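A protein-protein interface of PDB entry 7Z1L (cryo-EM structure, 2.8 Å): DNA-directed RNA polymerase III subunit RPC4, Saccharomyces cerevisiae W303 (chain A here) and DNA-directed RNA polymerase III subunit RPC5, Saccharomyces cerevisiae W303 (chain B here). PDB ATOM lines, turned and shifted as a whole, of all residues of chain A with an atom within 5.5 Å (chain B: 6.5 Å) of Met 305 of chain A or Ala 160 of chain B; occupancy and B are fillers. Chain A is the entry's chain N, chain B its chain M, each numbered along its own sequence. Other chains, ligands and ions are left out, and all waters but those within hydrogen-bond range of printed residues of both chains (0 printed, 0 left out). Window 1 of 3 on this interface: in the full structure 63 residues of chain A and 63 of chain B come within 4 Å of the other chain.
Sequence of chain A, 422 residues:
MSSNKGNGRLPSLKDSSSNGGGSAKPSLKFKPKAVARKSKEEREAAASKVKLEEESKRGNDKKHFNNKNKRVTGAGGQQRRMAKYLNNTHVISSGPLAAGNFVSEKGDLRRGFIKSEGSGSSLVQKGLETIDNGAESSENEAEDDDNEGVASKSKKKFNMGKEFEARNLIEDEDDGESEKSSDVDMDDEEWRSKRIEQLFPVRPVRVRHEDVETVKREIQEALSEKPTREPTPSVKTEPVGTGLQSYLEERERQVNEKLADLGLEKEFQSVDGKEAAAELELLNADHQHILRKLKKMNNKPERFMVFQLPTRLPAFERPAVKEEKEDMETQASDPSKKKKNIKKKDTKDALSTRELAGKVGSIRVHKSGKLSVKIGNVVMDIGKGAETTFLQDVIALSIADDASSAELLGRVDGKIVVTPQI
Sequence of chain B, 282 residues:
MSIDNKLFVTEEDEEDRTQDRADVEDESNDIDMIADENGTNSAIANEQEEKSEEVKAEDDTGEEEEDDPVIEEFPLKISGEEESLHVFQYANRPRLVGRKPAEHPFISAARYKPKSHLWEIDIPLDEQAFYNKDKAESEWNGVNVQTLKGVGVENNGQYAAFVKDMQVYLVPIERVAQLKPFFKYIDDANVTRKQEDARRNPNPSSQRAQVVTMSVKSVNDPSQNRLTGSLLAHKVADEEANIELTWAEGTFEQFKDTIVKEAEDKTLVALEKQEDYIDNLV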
ATOM      1  N   LYS A 293       1.296   1.650  25.915  1.00  0.00           N
ATOM      2  CA  LYS A 293       2.374   1.624  24.932  1.00  0.00           C
ATOM      3  C   LYS A 293       2.534   0.236  24.323  1.00  0.00           C
ATOM      4  O   LYS A 293       2.873   0.107  23.141  1.00  0.00           O
ATOM      5  CB  LYS A 293       3.680   2.088  25.575  1.00  0.00           C
ATOM      6  CG  LYS A 293       4.779   2.408  24.578  1.00  0.00           C
ATOM      7  CD  LYS A 293       6.046   2.881  25.271  1.00  0.00           C
ATOM      8  CE  LYS A 293       5.948   4.344  25.661  1.00  0.00           C
ATOM      9  NZ  LYS A 293       5.988   5.238  24.471  1.00  0.00           N
ATOM     10  N   LEU A 294       2.296  -0.815  25.112  1.00  0.00           N
ATOM     11  CA  LEU A 294       2.304  -2.168  24.568  1.00  0.00           C
ATOM     12  C   LEU A 294       1.143  -2.379  23.608  1.00  0.00           C
ATOM     13  O   LEU A 294       1.295  -3.046  22.578  1.00  0.00           O
ATOM     14  CB  LEU A 294       2.253  -3.191  25.702  1.00  0.00           C
ATOM     15  CG  LEU A 294       3.595  -3.708  26.221  1.00  0.00           C
ATOM     16  CD1 LEU A 294       3.387  -4.620  27.413  1.00  0.00           C
ATOM     17  CD2 LEU A 294       4.331  -4.436  25.114  1.00  0.00           C
ATOM     18  N   MET A 297       1.837  -0.447  19.951  1.00  0.00           N
ATOM     19  CA  MET A 297       2.793  -0.951  18.971  1.00  0.00           C
ATOM     20  C   MET A 297       2.461  -2.356  18.474  1.00  0.00           C
ATOM     21  O   MET A 297       3.370  -3.093  18.067  1.00  0.00           O
ATOM     22  CB  MET A 297       4.215  -0.907  19.536  1.00  0.00           C
ATOM     23  CG  MET A 297       4.470  -1.807  20.735  1.00  0.00           C
ATOM     24  SD  MET A 297       6.141  -1.612  21.379  1.00  0.00           S
ATOM     25  CE  MET A 297       6.027  -0.013  22.168  1.00  0.00           C
ATOM     26  N   ARG A 303       9.333  -1.100  15.030  1.00  0.00           N
ATOM     27  CA  ARG A 303       9.007  -0.552  16.344  1.00  0.00           C
ATOM     28  C   ARG A 303       9.503  -1.530  17.401  1.00  0.00           C
ATOM     29  O   ARG A 303       8.976  -2.641  17.518  1.00  0.00           O
ATOM     30  CB  ARG A 303       7.505  -0.311  16.486  1.00  0.00           C
ATOM     31  CG  ARG A 303       7.019   0.999  15.888  1.00  0.00           C
ATOM     32  CD  ARG A 303       7.303   2.180  16.800  1.00  0.00           C
ATOM     33  NE  ARG A 303       7.605   3.386  16.037  1.00  0.00           N
ATOM     34  CZ  ARG A 303       7.900   4.562  16.574  1.00  0.00           C
ATOM     35  NH1 ARG A 303       7.962   4.727  17.885  1.00  0.00           N
ATOM     36  NH2 ARG A 303       8.139   5.598  15.775  1.00  0.00           N
ATOM     37  N   PHE A 304      10.508  -1.119  18.168  1.00  0.00           N
ATOM     38  CA  PHE A 304      11.122  -1.962  19.181  1.00  0.00           C
ATOM     39  C   PHE A 304      11.027  -1.296  20.546  1.00  0.00           C
ATOM     40  O   PHE A 304      10.963  -0.067  20.653  1.00  0.00           O
ATOM     41  CB  PHE A 304      12.591  -2.244  18.854  1.00  0.00           C
ATOM     42  CG  PHE A 304      12.793  -3.384  17.905  1.00  0.00           C
ATOM     43  CD1 PHE A 304      12.589  -3.215  16.548  1.00  0.00           C
ATOM     44  CD2 PHE A 304      13.195  -4.625  18.367  1.00  0.00           C
ATOM     45  CE1 PHE A 304      12.780  -4.261  15.671  1.00  0.00           C
ATOM     46  CE2 PHE A 304      13.386  -5.676  17.493  1.00  0.00           C
ATOM     47  CZ  PHE A 304      13.178  -5.492  16.143  1.00  0.00           C
ATOM     48  N   MET A 305      11.014  -2.121  21.589  1.00  0.00           N
ATOM     49  CA  MET A 305      11.042  -1.641  22.962  1.00  0.00           C
ATOM     50  C   MET A 305      11.962  -2.549  23.765  1.00  0.00           C
ATOM     51  O   MET A 305      11.879  -3.776  23.659  1.00  0.00           O
ATOM     52  CB  MET A 305       9.633  -1.601  23.568  1.00  0.00           C
ATOM     53  CG  MET A 305       9.574  -1.061  24.981  1.00  0.00           C
ATOM     54  SD  MET A 305       7.892  -1.004  25.628  1.00  0.00           S
ATOM     55  CE  MET A 305       7.562  -2.743  25.877  1.00  0.00           C
ATOM     56  N   VAL A 306      12.836  -1.945  24.563  1.00  0.00           N
ATOM     57  CA  VAL A 306      13.932  -2.668  25.199  1.00  0.00           C
ATOM     58  C   VAL A 306      13.482  -3.180  26.562  1.00  0.00           C
ATOM     59  O   VAL A 306      13.094  -2.398  27.437  1.00  0.00           O
ATOM     60  CB  VAL A 306      15.181  -1.782  25.328  1.00  0.00           C
ATOM     61  CG1 VAL A 306      16.165  -2.383  26.319  1.00  0.00           C
ATOM     62  CG2 VAL A 306      15.842  -1.615  23.976  1.00  0.00           C
ATOM     63  N   PHE A 307      13.546  -4.495  26.739  1.00  0.00           N
ATOM     64  CA  PHE A 307      13.297  -5.137  28.019  1.00  0.00           C
ATOM     65  C   PHE A 307      14.593  -5.221  28.815  1.00  0.00           C
ATOM     66  O   PHE A 307      15.682  -5.347  28.251  1.00  0.00           O
ATOM     67  CB  PHE A 307      12.733  -6.543  27.814  1.00  0.00           C
ATOM     68  CG  PHE A 307      11.242  -6.596  27.638  1.00  0.00           C
ATOM     69  CD1 PHE A 307      10.592  -5.726  26.782  1.00  0.00           C
ATOM     70  CD2 PHE A 307      10.492  -7.552  28.303  1.00  0.00           C
ATOM     71  CE1 PHE A 307       9.223  -5.793  26.612  1.00  0.00           C
ATOM     72  CE2 PHE A 307       9.126  -7.627  28.134  1.00  0.00           C
ATOM     73  CZ  PHE A 307       8.490  -6.746  27.286  1.00  0.00           C
ATOM     74  N   VAL A 394      17.862  -0.369  16.571  1.00  0.00           N
ATOM     75  CA  VAL A 394      18.406  -1.720  16.648  1.00  0.00           C
ATOM     76  C   VAL A 394      19.087  -2.046  15.327  1.00  0.00           C
ATOM     77  O   VAL A 394      18.542  -1.771  14.251  1.00  0.00           O
ATOM     78  CB  VAL A 394      17.313  -2.748  16.988  1.00  0.00           C
ATOM     79  CG1 VAL A 394      16.933  -2.641  18.453  1.00  0.00           C
ATOM     80  CG2 VAL A 394      16.086  -2.546  16.117  1.00  0.00           C
ATOM     81  N   ARG A 411      13.505   1.367  15.393  1.00  0.00           N
ATOM     82  CA  ARG A 411      13.908   2.293  16.440  1.00  0.00           C
ATOM     83  C   ARG A 411      13.368   1.828  17.785  1.00  0.00           C
ATOM     84  O   ARG A 411      12.293   1.226  17.862  1.00  0.00           O
ATOM     85  CB  ARG A 411      13.418   3.714  16.141  1.00  0.00           C
ATOM     86  CG  ARG A 411      11.903   3.869  16.117  1.00  0.00           C
ATOM     87  CD  ARG A 411      11.479   5.318  15.888  1.00  0.00           C
ATOM     88  NE  ARG A 411      12.329   6.040  14.947  1.00  0.00           N
ATOM     89  CZ  ARG A 411      12.370   5.826  13.637  1.00  0.00           C
ATOM     90  NH1 ARG A 411      11.590   4.929  13.055  1.00  0.00           N
ATOM     91  NH2 ARG A 411      13.208   6.539  12.891  1.00  0.00           N
ATOM     92  N   VAL A 412      14.133   2.092  18.844  1.00  0.00           N
ATOM     93  CA  VAL A 412      13.695   1.743  20.189  1.00  0.00           C
ATOM     94  C   VAL A 412      12.780   2.838  20.716  1.00  0.00           C
ATOM     95  O   VAL A 412      13.157   4.016  20.768  1.00  0.00           O
ATOM     96  CB  VAL A 412      14.905   1.532  21.110  1.00  0.00           C
ATOM     97  CG1 VAL A 412      14.478   1.560  22.570  1.00  0.00           C
ATOM     98  CG2 VAL A 412      15.603   0.226  20.776  1.00  0.00           C
ATOM     99  N   ASP A 413      11.567   2.455  21.107  1.00  0.00           N
ATOM    100  CA  ASP A 413      10.570   3.382  21.635  1.00  0.00           C
ATOM    101  C   ASP A 413      10.274   2.969  23.073  1.00  0.00           C
ATOM    102  O   ASP A 413       9.356   2.187  23.332  1.00  0.00           O
ATOM    103  CB  ASP A 413       9.306   3.380  20.775  1.00  0.00           C
ATOM    104  CG  ASP A 413       8.389   4.551  21.079  1.00  0.00           C
ATOM    105  OD1 ASP A 413       8.737   5.380  21.946  1.00  0.00           O
ATOM    106  OD2 ASP A 413       7.317   4.643  20.445  1.00  0.00           O
ATOM    107  N   GLY A 414      11.054   3.502  24.009  1.00  0.00           N
ATOM    108  CA  GLY A 414      10.853   3.214  25.413  1.00  0.00           C
ATOM    109  C   GLY A 414      11.683   2.049  25.910  1.00  0.00           C
ATOM    110  O   GLY A 414      12.424   1.392  25.174  1.00  0.00           O
ATOM    111  N   LYS A 415      11.543   1.794  27.207  1.00  0.00           N
ATOM    112  CA  LYS A 415      12.285   0.742  27.887  1.00  0.00           C
ATOM    113  C   LYS A 415      11.493   0.324  29.117  1.00  0.00           C
ATOM    114  O   LYS A 415      10.855   1.154  29.765  1.00  0.00           O
ATOM    115  CB  LYS A 415      13.692   1.224  28.273  1.00  0.00           C
ATOM    116  CG  LYS A 415      14.443   0.334  29.253  1.00  0.00           C
ATOM    117  CD  LYS A 415      15.944   0.442  29.065  1.00  0.00           C
ATOM    118  CE  LYS A 415      16.673  -0.583  29.914  1.00  0.00           C
ATOM    119  NZ  LYS A 415      17.862  -1.131  29.211  1.00  0.00           N
ATOM    120  N   ILE A 416      11.512  -0.975  29.420  1.00  0.00           N
ATOM    121  CA  ILE A 416      10.910  -1.482  30.646  1.00  0.00           C
ATOM    122  C   ILE A 416      11.940  -2.310  31.404  1.00  0.00           C
ATOM    123  O   ILE A 416      12.903  -2.828  30.835  1.00  0.00           O
ATOM    124  CB  ILE A 416       9.637  -2.321  30.408  1.00  0.00           C
ATOM    125  CG1 ILE A 416       9.986  -3.660  29.773  1.00  0.00           C
ATOM    126  CG2 ILE A 416       8.640  -1.566  29.542  1.00  0.00           C
ATOM    127  CD1 ILE A 416       8.977  -4.714  30.080  1.00  0.00           C
ATOM    128  N   LEU B  85      22.139  -8.970  17.686  1.00  0.00           N
ATOM    129  CA  LEU B  85      21.433  -7.708  17.516  1.00  0.00           C
ATOM    130  C   LEU B  85      22.081  -6.623  18.368  1.00  0.00           C
ATOM    131  O   LEU B  85      22.199  -6.771  19.587  1.00  0.00           O
ATOM    132  CB  LEU B  85      19.963  -7.874  17.897  1.00  0.00           C
ATOM    133  CG  LEU B  85      19.040  -6.666  17.744  1.00  0.00           C
ATOM    134  CD1 LEU B  85      19.171  -6.059  16.361  1.00  0.00           C
ATOM    135  CD2 LEU B  85      17.603  -7.069  18.020  1.00  0.00           C
ATOM    136  N   VAL B  87      22.456  -2.315  19.417  1.00  0.00           N
ATOM    137  CA  VAL B  87      21.642  -1.131  19.659  1.00  0.00           C
ATOM    138  C   VAL B  87      22.537   0.096  19.576  1.00  0.00           C
ATOM    139  O   VAL B  87      23.561   0.176  20.263  1.00  0.00           O
ATOM    140  CB  VAL B  87      20.930  -1.196  21.028  1.00  0.00           C
ATOM    141  CG1 VAL B  87      20.399   0.171  21.421  1.00  0.00           C
ATOM    142  CG2 VAL B  87      19.803  -2.208  20.991  1.00  0.00           C
ATOM    143  N   GLN B 158      19.692  -7.478  28.535  1.00  0.00           N
ATOM    144  CA  GLN B 158      18.948  -6.542  27.704  1.00  0.00           C
ATOM    145  C   GLN B 158      18.339  -7.285  26.525  1.00  0.00           C
ATOM    146  O   GLN B 158      19.047  -7.983  25.792  1.00  0.00           O
ATOM    147  CB  GLN B 158      19.853  -5.416  27.203  1.00  0.00           C
ATOM    148  CG  GLN B 158      20.698  -4.765  28.281  1.00  0.00           C
ATOM    149  CD  GLN B 158      19.868  -4.041  29.321  1.00  0.00           C
ATOM    150  OE1 GLN B 158      18.783  -3.539  29.027  1.00  0.00           O
ATOM    151  NE2 GLN B 158      20.375  -3.983  30.546  1.00  0.00           N
ATOM    152  N   TYR B 159      17.028  -7.135  26.346  1.00  0.00           N
ATOM    153  CA  TYR B 159      16.309  -7.766  25.250  1.00  0.00           C
ATOM    154  C   TYR B 159      15.553  -6.707  24.467  1.00  0.00           C
ATOM    155  O   TYR B 159      14.848  -5.882  25.056  1.00  0.00           O
ATOM    156  CB  TYR B 159      15.331  -8.828  25.761  1.00  0.00           C
ATOM    157  CG  TYR B 159      15.971  -9.975  26.507  1.00  0.00           C
ATOM    158  CD1 TYR B 159      16.448 -11.089  25.832  1.00  0.00           C
ATOM    159  CD2 TYR B 159      16.087  -9.949  27.889  1.00  0.00           C
ATOM    160  CE1 TYR B 159      17.030 -12.140  26.512  1.00  0.00           C
ATOM    161  CE2 TYR B 159      16.667 -10.995  28.576  1.00  0.00           C
ATOM    162  CZ  TYR B 159      17.137 -12.088  27.883  1.00  0.00           C
ATOM    163  OH  TYR B 159      17.716 -13.131  28.566  1.00  0.00           O
ATOM    164  N   ALA B 160      15.698  -6.732  23.144  1.00  0.00           N
ATOM    165  CA  ALA B 160      14.885  -5.896  22.275  1.00  0.00           C
ATOM    166  C   ALA B 160      13.617  -6.651  21.908  1.00  0.00           C
ATOM    167  O   ALA B 160      13.681  -7.780  21.415  1.00  0.00           O
ATOM    168  CB  ALA B 160      15.661  -5.510  21.017  1.00  0.00           C
ATOM    169  N   ALA B 161      12.465  -6.041  22.157  1.00  0.00           N
ATOM    170  CA  ALA B 161      11.194  -6.740  22.062  1.00  0.00           C
ATOM    171  C   ALA B 161      10.247  -6.028  21.112  1.00  0.00           C
ATOM    172  O   ALA B 161      10.221  -4.795  21.045  1.00  0.00           O
ATOM    173  CB  ALA B 161      10.534  -6.868  23.432  1.00  0.00           C
ATOM    174  N   PHE B 162       9.467  -6.820  20.382  1.00  0.00           N
ATOM    175  CA  PHE B 162       8.370  -6.315  19.568  1.00  0.00           C
ATOM    176  C   PHE B 162       7.102  -7.087  19.916  1.00  0.00           C
ATOM    177  O   PHE B 162       7.120  -8.025  20.717  1.00  0.00           O
ATOM    178  CB  PHE B 162       8.695  -6.395  18.069  1.00  0.00           C
ATOM    179  CG  PHE B 162       8.967  -7.784  17.568  1.00  0.00           C
ATOM    180  CD1 PHE B 162      10.250  -8.303  17.594  1.00  0.00           C
ATOM    181  CD2 PHE B 162       7.947  -8.558  17.041  1.00  0.00           C
ATOM    182  CE1 PHE B 162      10.505  -9.575  17.125  1.00  0.00           C
ATOM    183  CE2 PHE B 162       8.198  -9.829  16.571  1.00  0.00           C
ATOM    184  CZ  PHE B 162       9.477 -10.337  16.613  1.00  0.00           C
ATOM    185  N   VAL B 163       5.986  -6.679  19.316  1.00  0.00           N
ATOM    186  CA  VAL B 163       4.675  -7.235  19.624  1.00  0.00           C
ATOM    187  C   VAL B 163       4.068  -7.804  18.350  1.00  0.00           C
ATOM    188  O   VAL B 163       4.111  -7.168  17.292  1.00  0.00           O
ATOM    189  CB  VAL B 163       3.737  -6.176  20.245  1.00  0.00           C
ATOM    190  CG1 VAL B 163       2.450  -6.820  20.732  1.00  0.00           C
ATOM    191  CG2 VAL B 163       4.431  -5.453  21.385  1.00  0.00           C
ATOM    192  N   VAL B 168       4.543 -10.835  22.993  1.00  0.00           N
ATOM    193  CA  VAL B 168       5.755 -10.029  23.046  1.00  0.00           C
ATOM    194  C   VAL B 168       6.958 -10.932  22.814  1.00  0.00           C
ATOM    195  O   VAL B 168       7.231 -11.839  23.609  1.00  0.00           O
ATOM    196  CB  VAL B 168       5.871  -9.289  24.385  1.00  0.00           C
ATOM    197  CG1 VAL B 168       7.042  -8.326  24.355  1.00  0.00           C
ATOM    198  CG2 VAL B 168       4.579  -8.556  24.699  1.00  0.00           C
ATOM    199  N   TYR B 169       7.690 -10.667  21.738  1.00  0.00           N
ATOM    200  CA  TYR B 169       8.852 -11.449  21.348  1.00  0.00           C
ATOM    201  C   TYR B 169      10.116 -10.674  21.689  1.00  0.00           C
ATOM    202  O   TYR B 169      10.246  -9.498  21.328  1.00  0.00           O
ATOM    203  CB  TYR B 169       8.822 -11.776  19.853  1.00  0.00           C
ATOM    204  CG  TYR B 169       7.747 -12.761  19.448  1.00  0.00           C
ATOM    205  CD1 TYR B 169       6.415 -12.379  19.377  1.00  0.00           C
ATOM    206  CD2 TYR B 169       8.069 -14.073  19.132  1.00  0.00           C
ATOM    207  CE1 TYR B 169       5.434 -13.275  19.006  1.00  0.00           C
ATOM    208  CE2 TYR B 169       7.095 -14.976  18.759  1.00  0.00           C
ATOM    209  CZ  TYR B 169       5.780 -14.572  18.699  1.00  0.00           C
ATOM    210  OH  TYR B 169       4.807 -15.471  18.328  1.00  0.00           O
ATOM    211  N   LEU B 170      11.042 -11.342  22.371  1.00  0.00           N
ATOM    212  CA  LEU B 170      12.276 -10.750  22.859  1.00  0.00           C
ATOM    213  C   LEU B 170      13.470 -11.389  22.161  1.00  0.00           C
ATOM    214  O   LEU B 170      13.545 -12.611  22.015  1.00  0.00           O
ATOM    215  CB  LEU B 170      12.412 -10.944  24.373  1.00  0.00           C
ATOM    216  CG  LEU B 170      11.730 -10.008  25.375  1.00  0.00           C
ATOM    217  CD1 LEU B 170      10.217 -10.062  25.268  1.00  0.00           C
ATOM    218  CD2 LEU B 170      12.162 -10.369  26.784  1.00  0.00           C
ATOM    219  N   VAL B 171      14.405 -10.551  21.728  1.00  0.00           N
ATOM    220  CA  VAL B 171      15.647 -11.010  21.115  1.00  0.00           C
ATOM    221  C   VAL B 171      16.798 -10.466  21.951  1.00  0.00           C
ATOM    222  O   VAL B 171      16.795  -9.272  22.290  1.00  0.00           O
ATOM    223  CB  VAL B 171      15.753 -10.562  19.649  1.00  0.00           C
ATOM    224  CG1 VAL B 171      16.991 -11.149  18.996  1.00  0.00           C
ATOM    225  CG2 VAL B 171      14.505 -10.961  18.878  1.00  0.00           C
ATOM    226  N   PRO B 172      17.773 -11.291  22.333  1.00  0.00           N
ATOM    227  CA  PRO B 172      18.885 -10.792  23.150  1.00  0.00           C
ATOM    228  C   PRO B 172      19.697  -9.728  22.426  1.00  0.00           C
ATOM    229  O   PRO B 172      19.942  -9.817  21.221  1.00  0.00           O
ATOM    230  CB  PRO B 172      19.722 -12.049  23.415  1.00  0.00           C
ATOM    231  CG  PRO B 172      18.765 -13.178  23.257  1.00  0.00           C
ATOM    232  CD  PRO B 172      17.814 -12.755  22.182  1.00  0.00           C
ATOM    233  N   ILE B 173      20.113  -8.716  23.179  1.00  0.00           N
ATOM    234  CA  ILE B 173      20.930  -7.625  22.665  1.00  0.00           C
ATOM    235  C   ILE B 173      22.379  -7.924  23.018  1.00  0.00           C
ATOM    236  O   ILE B 173      22.712  -8.120  24.193  1.00  0.00           O
ATOM    237  CB  ILE B 173      20.488  -6.272  23.241  1.00  0.00           C
ATOM    238  CG1 ILE B 173      19.088  -5.913  22.745  1.00  0.00           C
ATOM    239  CG2 ILE B 173      21.475  -5.185  22.861  1.00  0.00           C
ATOM    240  CD1 ILE B 173      18.492  -4.706  23.431  1.00  0.00           C
ATOM    241  N   PHE B 255      13.313 -10.635   9.424  1.00  0.00           N
ATOM    242  CA  PHE B 255      13.724 -10.851  10.807  1.00  0.00           C
ATOM    243  C   PHE B 255      12.533 -11.226  11.682  1.00  0.00           C
ATOM    244  O   PHE B 255      12.610 -12.158  12.492  1.00  0.00           O
ATOM    245  CB  PHE B 255      14.420  -9.594  11.330  1.00  0.00           C
ATOM    246  CG  PHE B 255      14.638  -9.584  12.814  1.00  0.00           C
ATOM    247  CD1 PHE B 255      15.653 -10.332  13.382  1.00  0.00           C
ATOM    248  CD2 PHE B 255      13.840  -8.806  13.639  1.00  0.00           C
ATOM    249  CE1 PHE B 255      15.861 -10.317  14.747  1.00  0.00           C
ATOM    250  CE2 PHE B 255      14.043  -8.789  15.003  1.00  0.00           C
ATOM    251  CZ  PHE B 255      15.055  -9.545  15.557  1.00  0.00           C
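The backbone carbonyl oxygen (O) of Met 305 of chain A sits at hydrogen-bond distance from the backbone NH (N) of Ala 161 of chain B, 2.8 Å away.
The backbone carbonyl oxygen (O) of Tyr 159 of chain B sits at hydrogen-bond distance from the backbone NH (N) of Phe 307 of chain A (2.5 Å).
The side-chain amide oxygen of Gln 158 of chain B sits at hydrogen-bond distance from the side-chain amino group of Lys 415 of chain A.
The backbone carbonyl oxygen (O) of Phe 162 of chain B lies within hydrogen-bond range of the backbone NH (N) of Tyr 169 of chain B.
The backbone carbonyl oxygen of Ala 160 of chain B lies within hydrogen-bond range of the backbone NH of Val 171 of chain B (2.9 Å).
N of Val 306 of chain A lies within hydrogen-bond range of O of Gly 414 of chain A (3.4 Å).
The backbone carbonyl oxygen (O) of Gln 158 of chain B is in hydrogen-bond range of the backbone NH (N) of Ile 173 of chain B (2.9 Å).
O of Phe 304 of chain A sits at hydrogen-bond distance from N of Asp 413 of chain A.
The side-chain carboxylate (OD2) of Asp 413 of chain A lies within salt-bridge range of the guanidinium group (NH1) of Arg 303 of chain A, 2.6 Å away.
Among the printed residues, merely in contact across the chains: Val 306 of chain A with Tyr 159 of chain B (3.3 Å), Phe 304 of chain A with Ala 161 of chain B (3.5 Å), Phe 307 of chain A with Gln 158 of chain B (3.5 Å), Phe 307 of chain A with Ala 161 of chain B (3.5 Å), Phe 304 of chain A with Phe 255 of chain B (3.6 Å), Phe 307 of chain A with Leu 170 of chain B (3.6 Å), Phe 307 of chain A with Val 168 of chain B (3.6 Å), Met 297 of chain A with Val 163 of chain B (3.7 Å), Phe 304 of chain A with Ala 160 of chain B (3.7 Å), Met 305 of chain A with Ala 160 of chain B (3.8 Å), Arg 303 of chain A with Phe 162 of chain B (3.8 Å), Val 394 of chain A with Leu 85 of chain B (3.8 Å), Val 394 of chain A with Val 87 of chain B (3.9 Å), Leu 294 of chain A with Val 163 of chain B (3.9 Å), Met 305 of chain A with Tyr 159 of chain B (3.9 Å) and Val 306 of chain A with Gln 158 of chain B (3.9 Å).
Of the printed residues of chain B, Met 305 of chain A touches Tyr 159, Ala 160 and Ala 161.
Ala 160 of chain B touches just these residues of chain A: Phe 304 and Met 305.
Of the printed residues of chain B, Arg 303 of chain A touches Phe 162.
Of the printed residues of chain A, Gln 158 of chain B touches Val 306, Phe 307 and Lys 415.
Of the 15 printed residues of chain A, 9 touch a printed residue of chain B.
Printed residues of chain A that touch a printed residue of chain B: Leu 294, Met 297, Arg 303, Phe 304, Met 305, Val 306, Phe 307, Val 394 and Lys 415.
Hydrophobic or aromatic side chains of chain A within 4 Å of the printed part of chain B: Leu 294, Met 297, Phe 304, Val 306, Phe 307 and Val 394.
Hydrophobic or aromatic side chains of chain B within 4 Å of the printed part of chain A: Leu 85, Val 87, Ala 160, Ala 161, Phe 162, Val 163, Val 168, Leu 170 and Phe 255.
Among the printed residues, 19 pairs touch across the chains.
Among the printed residues, no Asp or Glu carboxylate lies within 4 Å of a Lys or Arg side-chain nitrogen of the other chain.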
